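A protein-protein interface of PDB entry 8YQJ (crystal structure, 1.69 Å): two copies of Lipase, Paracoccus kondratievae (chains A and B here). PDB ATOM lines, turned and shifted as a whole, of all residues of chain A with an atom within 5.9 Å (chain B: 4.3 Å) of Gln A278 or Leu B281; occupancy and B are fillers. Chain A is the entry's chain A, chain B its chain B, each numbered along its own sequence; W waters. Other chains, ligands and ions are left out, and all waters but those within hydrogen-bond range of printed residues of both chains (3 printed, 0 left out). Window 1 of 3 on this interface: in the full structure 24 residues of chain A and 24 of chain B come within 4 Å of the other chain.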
ATOM      1  N   ALA A 273      21.395   8.148  31.212  1.00  0.00           N
ATOM      2  CA  ALA A 273      20.922   9.203  30.321  1.00  0.00           C
ATOM      3  C   ALA A 273      22.053   9.756  29.468  1.00  0.00           C
ATOM      4  O   ALA A 273      21.857  10.057  28.288  1.00  0.00           O
ATOM      5  CB  ALA A 273      20.276  10.334  31.126  1.00  0.00           C
ATOM      6  N   ARG A 274      23.239   9.923  30.046  1.00  0.00           N
ATOM      7  CA  ARG A 274      24.375  10.368  29.247  1.00  0.00           C
ATOM      8  C   ARG A 274      24.663   9.399  28.094  1.00  0.00           C
ATOM      9  O   ARG A 274      24.851   9.827  26.948  1.00  0.00           O
ATOM     10  CB  ARG A 274      25.589  10.563  30.148  1.00  0.00           C
ATOM     11  CG  ARG A 274      26.778  11.116  29.402  1.00  0.00           C
ATOM     12  CD  ARG A 274      27.905  11.406  30.344  1.00  0.00           C
ATOM     13  NE  ARG A 274      28.208  10.222  31.138  1.00  0.00           N
ATOM     14  CZ  ARG A 274      28.928   9.204  30.697  1.00  0.00           C
ATOM     15  NH1 ARG A 274      29.425   9.189  29.474  1.00  0.00           N
ATOM     16  NH2 ARG A 274      29.176   8.186  31.514  1.00  0.00           N
ATOM     17  N   ARG A 275      24.680   8.082  28.369  1.00  0.00           N
ATOM     18  CA  ARG A 275      24.916   7.107  27.297  1.00  0.00           C
ATOM     19  C   ARG A 275      23.803   7.152  26.258  1.00  0.00           C
ATOM     20  O   ARG A 275      24.061   6.991  25.051  1.00  0.00           O
ATOM     21  CB  ARG A 275      25.051   5.692  27.881  1.00  0.00           C
ATOM     22  CG  ARG A 275      26.378   5.475  28.615  1.00  0.00           C
ATOM     23  CD  ARG A 275      26.633   3.981  28.828  1.00  0.00           C
ATOM     24  NE  ARG A 275      25.443   3.356  29.387  1.00  0.00           N
ATOM     25  CZ  ARG A 275      25.228   3.149  30.680  1.00  0.00           C
ATOM     26  NH1 ARG A 275      26.120   3.482  31.598  1.00  0.00           N
ATOM     27  NH2 ARG A 275      24.081   2.601  31.062  1.00  0.00           N
ATOM     28  N   SER A 276      22.572   7.439  26.689  1.00  0.00           N
ATOM     29  CA  SER A 276      21.475   7.470  25.737  1.00  0.00           C
ATOM     30  C   SER A 276      21.658   8.619  24.765  1.00  0.00           C
ATOM     31  O   SER A 276      21.549   8.448  23.543  1.00  0.00           O
ATOM     32  CB  SER A 276      20.137   7.586  26.459  1.00  0.00           C
ATOM     33  OG  SER A 276      19.066   7.434  25.527  1.00  0.00           O
ATOM     34  N   PHE A 277      22.000   9.787  25.289  1.00  0.00           N
ATOM     35  CA  PHE A 277      22.207  10.906  24.385  1.00  0.00           C
ATOM     36  C   PHE A 277      23.408  10.634  23.489  1.00  0.00           C
ATOM     37  O   PHE A 277      23.424  11.051  22.331  1.00  0.00           O
ATOM     38  CB  PHE A 277      22.406  12.180  25.190  1.00  0.00           C
ATOM     39  CG  PHE A 277      22.343  13.439  24.360  1.00  0.00           C
ATOM     40  CD1 PHE A 277      21.230  13.723  23.577  1.00  0.00           C
ATOM     41  CD2 PHE A 277      23.404  14.326  24.362  1.00  0.00           C
ATOM     42  CE1 PHE A 277      21.190  14.888  22.804  1.00  0.00           C
ATOM     43  CE2 PHE A 277      23.370  15.469  23.604  1.00  0.00           C
ATOM     44  CZ  PHE A 277      22.267  15.761  22.845  1.00  0.00           C
ATOM     45  N   GLN A 278      24.416   9.930  24.012  1.00  0.00           N
ATOM     46  CA  GLN A 278      25.545   9.546  23.175  1.00  0.00           C
ATOM     47  C   GLN A 278      25.081   8.680  22.012  1.00  0.00           C
ATOM     48  O   GLN A 278      25.520   8.872  20.881  1.00  0.00           O
ATOM     49  CB  GLN A 278      26.612   8.843  24.018  1.00  0.00           C
ATOM     50  CG  GLN A 278      27.451   9.861  24.799  1.00  0.00           C
ATOM     51  CD  GLN A 278      28.331   9.254  25.862  1.00  0.00           C
ATOM     52  OE1 GLN A 278      28.919   9.986  26.655  1.00  0.00           O
ATOM     53  NE2 GLN A 278      28.397   7.924  25.911  1.00  0.00           N
ATOM     54  N   ALA A 279      24.129   7.772  22.252  1.00  0.00           N
ATOM     55  CA  ALA A 279      23.619   6.956  21.157  1.00  0.00           C
ATOM     56  C   ALA A 279      22.756   7.774  20.209  1.00  0.00           C
ATOM     57  O   ALA A 279      22.821   7.594  18.986  1.00  0.00           O
ATOM     58  CB  ALA A 279      22.823   5.774  21.714  1.00  0.00           C
ATOM     59  N   ILE A 280      21.943   8.680  20.750  1.00  0.00           N
ATOM     60  CA  ILE A 280      21.154   9.557  19.886  1.00  0.00           C
ATOM     61  C   ILE A 280      22.066  10.352  18.947  1.00  0.00           C
ATOM     62  O   ILE A 280      21.788  10.467  17.749  1.00  0.00           O
ATOM     63  CB  ILE A 280      20.268  10.486  20.739  1.00  0.00           C
ATOM     64  CG1 ILE A 280      19.174   9.674  21.428  1.00  0.00           C
ATOM     65  CG2 ILE A 280      19.672  11.657  19.876  1.00  0.00           C
ATOM     66  CD1 ILE A 280      18.594  10.319  22.666  1.00  0.00           C
ATOM     67  N   LEU A 281      23.178  10.891  19.463  1.00  0.00           N
ATOM     68  CA  LEU A 281      24.052  11.690  18.605  1.00  0.00           C
ATOM     69  C   LEU A 281      24.690  10.833  17.526  1.00  0.00           C
ATOM     70  O   LEU A 281      24.874  11.286  16.391  1.00  0.00           O
ATOM     71  CB  LEU A 281      25.136  12.387  19.431  1.00  0.00           C
ATOM     72  CG  LEU A 281      24.670  13.471  20.382  1.00  0.00           C
ATOM     73  CD1 LEU A 281      25.843  13.877  21.267  1.00  0.00           C
ATOM     74  CD2 LEU A 281      24.164  14.652  19.599  1.00  0.00           C
ATOM     75  N   SER A 282      25.021   9.578  17.849  1.00  0.00           N
ATOM     76  CA  SER A 282      25.570   8.700  16.828  1.00  0.00           C
ATOM     77  C   SER A 282      24.532   8.388  15.762  1.00  0.00           C
ATOM     78  O   SER A 282      24.855   8.352  14.571  1.00  0.00           O
ATOM     79  CB  SER A 282      26.097   7.415  17.461  1.00  0.00           C
ATOM     80  OG  SER A 282      27.054   7.717  18.455  1.00  0.00           O
ATOM     81  N   ALA A 283      23.278   8.173  16.168  1.00  0.00           N
ATOM     82  CA  ALA A 283      22.241   7.856  15.193  1.00  0.00           C
ATOM     83  C   ALA A 283      22.039   9.008  14.236  1.00  0.00           C
ATOM     84  O   ALA A 283      21.788   8.801  13.043  1.00  0.00           O
ATOM     85  CB  ALA A 283      20.920   7.531  15.891  1.00  0.00           C
ATOM     86  N   GLU B  94      31.425   2.461  26.355  1.00  0.00           N
ATOM     87  CA  GLU B  94      30.528   3.515  25.883  1.00  0.00           C
ATOM     88  C   GLU B  94      30.640   3.732  24.390  1.00  0.00           C
ATOM     89  O   GLU B  94      29.642   4.072  23.756  1.00  0.00           O
ATOM     90  CB  GLU B  94      30.763   4.826  26.634  1.00  0.00           C
ATOM     91  CG  GLU B  94      30.463   4.700  28.115  1.00  0.00           C
ATOM     92  CD  GLU B  94      30.528   6.012  28.863  1.00  0.00           C
ATOM     93  OE1 GLU B  94      30.689   7.066  28.217  1.00  0.00           O
ATOM     94  OE2 GLU B  94      30.470   5.980  30.106  1.00  0.00           O
ATOM     95  N   ILE B  95      31.815   3.534  23.788  1.00  0.00           N
ATOM     96  CA  ILE B  95      31.874   3.601  22.328  1.00  0.00           C
ATOM     97  C   ILE B  95      30.991   2.519  21.723  1.00  0.00           C
ATOM     98  O   ILE B  95      30.218   2.760  20.792  1.00  0.00           O
ATOM     99  CB  ILE B  95      33.325   3.492  21.825  1.00  0.00           C
ATOM    100  CG1 ILE B  95      34.140   4.707  22.283  1.00  0.00           C
ATOM    101  CG2 ILE B  95      33.355   3.407  20.296  1.00  0.00           C
ATOM    102  CD1 ILE B  95      35.669   4.517  22.223  1.00  0.00           C
ATOM    103  N   ALA B  98      27.203   3.326  22.222  1.00  0.00           N
ATOM    104  CA  ALA B  98      26.675   4.483  21.513  1.00  0.00           C
ATOM    105  C   ALA B  98      26.622   4.250  20.014  1.00  0.00           C
ATOM    106  O   ALA B  98      25.688   4.716  19.359  1.00  0.00           O
ATOM    107  CB  ALA B  98      27.523   5.719  21.822  1.00  0.00           C
ATOM    108  N   PHE B 277      33.657  14.227  24.394  1.00  0.00           N
ATOM    109  CA  PHE B 277      33.482  12.800  24.134  1.00  0.00           C
ATOM    110  C   PHE B 277      32.324  12.577  23.173  1.00  0.00           C
ATOM    111  O   PHE B 277      32.388  11.688  22.314  1.00  0.00           O
ATOM    112  CB  PHE B 277      33.253  12.047  25.444  1.00  0.00           C
ATOM    113  CG  PHE B 277      33.330  10.551  25.303  1.00  0.00           C
ATOM    114  CD1 PHE B 277      34.458   9.958  24.730  1.00  0.00           C
ATOM    115  CD2 PHE B 277      32.286   9.749  25.695  1.00  0.00           C
ATOM    116  CE1 PHE B 277      34.546   8.572  24.585  1.00  0.00           C
ATOM    117  CE2 PHE B 277      32.367   8.358  25.550  1.00  0.00           C
ATOM    118  CZ  PHE B 277      33.507   7.783  25.003  1.00  0.00           C
ATOM    119  N   GLN B 278      31.279  13.408  23.275  1.00  0.00           N
ATOM    120  CA  GLN B 278      30.175  13.335  22.319  1.00  0.00           C
ATOM    121  C   GLN B 278      30.654  13.591  20.889  1.00  0.00           C
ATOM    122  O   GLN B 278      30.191  12.931  19.947  1.00  0.00           O
ATOM    123  CB  GLN B 278      29.071  14.319  22.727  1.00  0.00           C
ATOM    124  CG  GLN B 278      28.246  13.785  23.922  1.00  0.00           C
ATOM    125  CD  GLN B 278      27.329  14.807  24.574  1.00  0.00           C
ATOM    126  OE1 GLN B 278      26.759  14.537  25.630  1.00  0.00           O
ATOM    127  NE2 GLN B 278      27.219  16.000  23.988  1.00  0.00           N
ATOM    128  N   ALA B 279      31.576  14.543  20.705  1.00  0.00           N
ATOM    129  CA  ALA B 279      32.109  14.806  19.369  1.00  0.00           C
ATOM    130  C   ALA B 279      33.030  13.678  18.923  1.00  0.00           C
ATOM    131  O   ALA B 279      33.041  13.308  17.743  1.00  0.00           O
ATOM    132  CB  ALA B 279      32.857  16.134  19.331  1.00  0.00           C
ATOM    133  N   ILE B 280      33.773  13.095  19.865  1.00  0.00           N
ATOM    134  CA  ILE B 280      34.636  11.965  19.533  1.00  0.00           C
ATOM    135  C   ILE B 280      33.808  10.787  19.033  1.00  0.00           C
ATOM    136  O   ILE B 280      34.178  10.109  18.066  1.00  0.00           O
ATOM    137  CB  ILE B 280      35.500  11.579  20.747  1.00  0.00           C
ATOM    138  CG1 ILE B 280      36.603  12.624  20.996  1.00  0.00           C
ATOM    139  CG2 ILE B 280      36.105  10.187  20.557  1.00  0.00           C
ATOM    140  CD1 ILE B 280      37.120  12.611  22.432  1.00  0.00           C
ATOM    141  N   LEU B 281      32.680  10.517  19.692  1.00  0.00           N
ATOM    142  CA  LEU B 281      31.817   9.417  19.263  1.00  0.00           C
ATOM    143  C   LEU B 281      31.226   9.675  17.881  1.00  0.00           C
ATOM    144  O   LEU B 281      31.141   8.757  17.046  1.00  0.00           O
ATOM    145  CB  LEU B 281      30.695   9.216  20.281  1.00  0.00           C
ATOM    146  CG  LEU B 281      31.156   8.696  21.626  1.00  0.00           C
ATOM    147  CD1 LEU B 281      29.994   8.743  22.618  1.00  0.00           C
ATOM    148  CD2 LEU B 281      31.726   7.302  21.490  1.00  0.00           C
ATOM    149  N   SER B 282      30.771  10.907  17.630  1.00  0.00           N
ATOM    150  CA  SER B 282      30.289  11.269  16.300  1.00  0.00           C
ATOM    151  C   SER B 282      31.364  11.049  15.250  1.00  0.00           C
ATOM    152  O   SER B 282      31.073  10.584  14.146  1.00  0.00           O
ATOM    153  CB  SER B 282      29.819  12.732  16.267  1.00  0.00           C
ATOM    154  OG  SER B 282      28.791  12.954  17.222  1.00  0.00           O
ATOM    155  N   ALA B 283      32.617  11.372  15.578  1.00  0.00           N
ATOM    156  CA  ALA B 283      33.683  11.214  14.596  1.00  0.00           C
ATOM    157  C   ALA B 283      33.932   9.745  14.319  1.00  0.00           C
ATOM    158  O   ALA B 283      34.185   9.352  13.173  1.00  0.00           O
ATOM    159  CB  ALA B 283      34.965  11.889  15.090  1.00  0.00           C
ATOM    160  N   ILE B 284      33.863   8.921  15.365  1.00  0.00           N
ATOM    161  CA  ILE B 284      34.022   7.488  15.161  1.00  0.00           C
ATOM    162  C   ILE B 284      32.899   6.965  14.288  1.00  0.00           C
ATOM    163  O   ILE B 284      33.124   6.205  13.334  1.00  0.00           O
ATOM    164  CB  ILE B 284      34.063   6.761  16.510  1.00  0.00           C
ATOM    165  CG1 ILE B 284      35.350   7.079  17.253  1.00  0.00           C
ATOM    166  CG2 ILE B 284      33.967   5.241  16.289  1.00  0.00           C
ATOM    167  CD1 ILE B 284      35.329   6.542  18.655  1.00  0.00           C
ATOM    168  N   MET B 285      31.670   7.397  14.581  1.00  0.00           N
ATOM    169  CA  MET B 285      30.520   6.937  13.817  1.00  0.00           C
ATOM    170  C   MET B 285      30.671   7.366  12.357  1.00  0.00           C
ATOM    171  O   MET B 285      30.422   6.588  11.432  1.00  0.00           O
ATOM    172  CB  MET B 285      29.244   7.560  14.374  1.00  0.00           C
ATOM    173  CG  MET B 285      27.906   6.855  14.075  1.00  0.00           C
ATOM    174  SD  MET B 285      27.851   5.040  14.330  1.00  0.00           S
ATOM    175  CE  MET B 285      28.567   4.314  12.863  1.00  0.00           C
HETATM  176  O   HOH W   1      27.564   5.440  25.168  1.00  0.00           O
HETATM  177  O   HOH W   2      28.828   4.414  31.671  1.00  0.00           O
HETATM  178  O   HOH W   3      23.304   4.734  17.990  1.00  0.00           O
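The side-chain hydroxyl (OG) of Ser A282 lies close to the backbone carbonyl oxygen (O) of Ala B98, 3.4 Å away. NH1 of Arg A274 lies within salt-bridge range of OE1 of Glu B94 (2.8 Å). The side-chain carboxylate (OE1) of Glu B94 is in hydrogen-bond range of the side-chain amide nitrogen (NE2) of Gln A278 (3.4 Å).
The side-chain hydroxyl of Ser B282 sits at hydrogen-bond distance from the backbone carbonyl oxygen of Gln B278 (3.1 Å). O of Gln A278 is in hydrogen-bond range of OG of Ser A282 (3.1 Å). The guanidinium group (NH1) of Arg A274 lies within hydrogen-bond range of the side-chain amide oxygen (OE1) of Gln A278 (3.0 Å).
Among the printed residues, pairs that only touch across the chains: Ser A282 with Met B285, Gln A278 with Phe B277, Gln A278 with Leu B281, Ala A279 with Ala B98, Leu A281 with Gln B278, Phe A277 with Gln B278, Gln A278 with Ala B98 and Arg A275 with Glu B94.
Of chain B, only Glu B94 (3.4 Å), Ala B98 (3.8 Å), Phe B277 (3.5 Å) and Leu B281 (3.5 Å) come within 4 Å of Gln A278. Of chain A, only Gln A278 (3.5 Å) comes within 4 Å of Leu B281. Of the printed residues of chain A, Phe B277 touches Gln A278. Printed residues of chain A within 4 Å of Ala B98: Gln A278, Ala A279 and Ser A282. Of the printed residues of chain B, Arg A275 touches Glu B94. Of the printed residues of chain B, Arg A274 touches Glu B94. Ile B284 touches none of the printed residues of chain A. Ile A280 touches none of the printed residues of chain B. The nearest residue of chain B that does not touch Gln A278 is Gln B278 (4.1 Å). The nearest printed residue of chain A that does not touch Met B285 is Ala A283 (5.2 Å).
Of the 11 printed residues of chain A, 7 touch a printed residue of chain B. Hydrophobic or aromatic side chains of chain A within 4 Å of the printed part of chain B: Phe A277, Ala A279 and Leu A281. Hydrophobic or aromatic side chains of chain B that line the printed part of chain A: Ala B98, Phe B277, Leu B281 and Met B285.
Phe A277 touches Gln B278, and with the chains exchanged Gln A278 touches Phe B277. Gln A278 touches Leu B281, and with the chains exchanged Leu A281 touches Gln B278. Positions printed for both chains: 277, 278, 279, 280, 281, 282 and 283. Of the 11 pairs that touch across the chains among the printed residues, 4 have their exchanged pair printed and touching as well.
Water W1 bridges the side-chain amide nitrogen (NE2) of Gln A278 and the backbone carbonyl oxygen (O) of Glu B94. Water W3 lies within hydrogen-bond range of O of Ala B98 (2.7 Å) and O of Ala A279 (3.1 Å). Water W2 bridges the side-chain carboxylate (OE2) of Glu B94 (2.8 Å) and the guanidinium group (NH1) of Arg A275 (2.9 Å).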
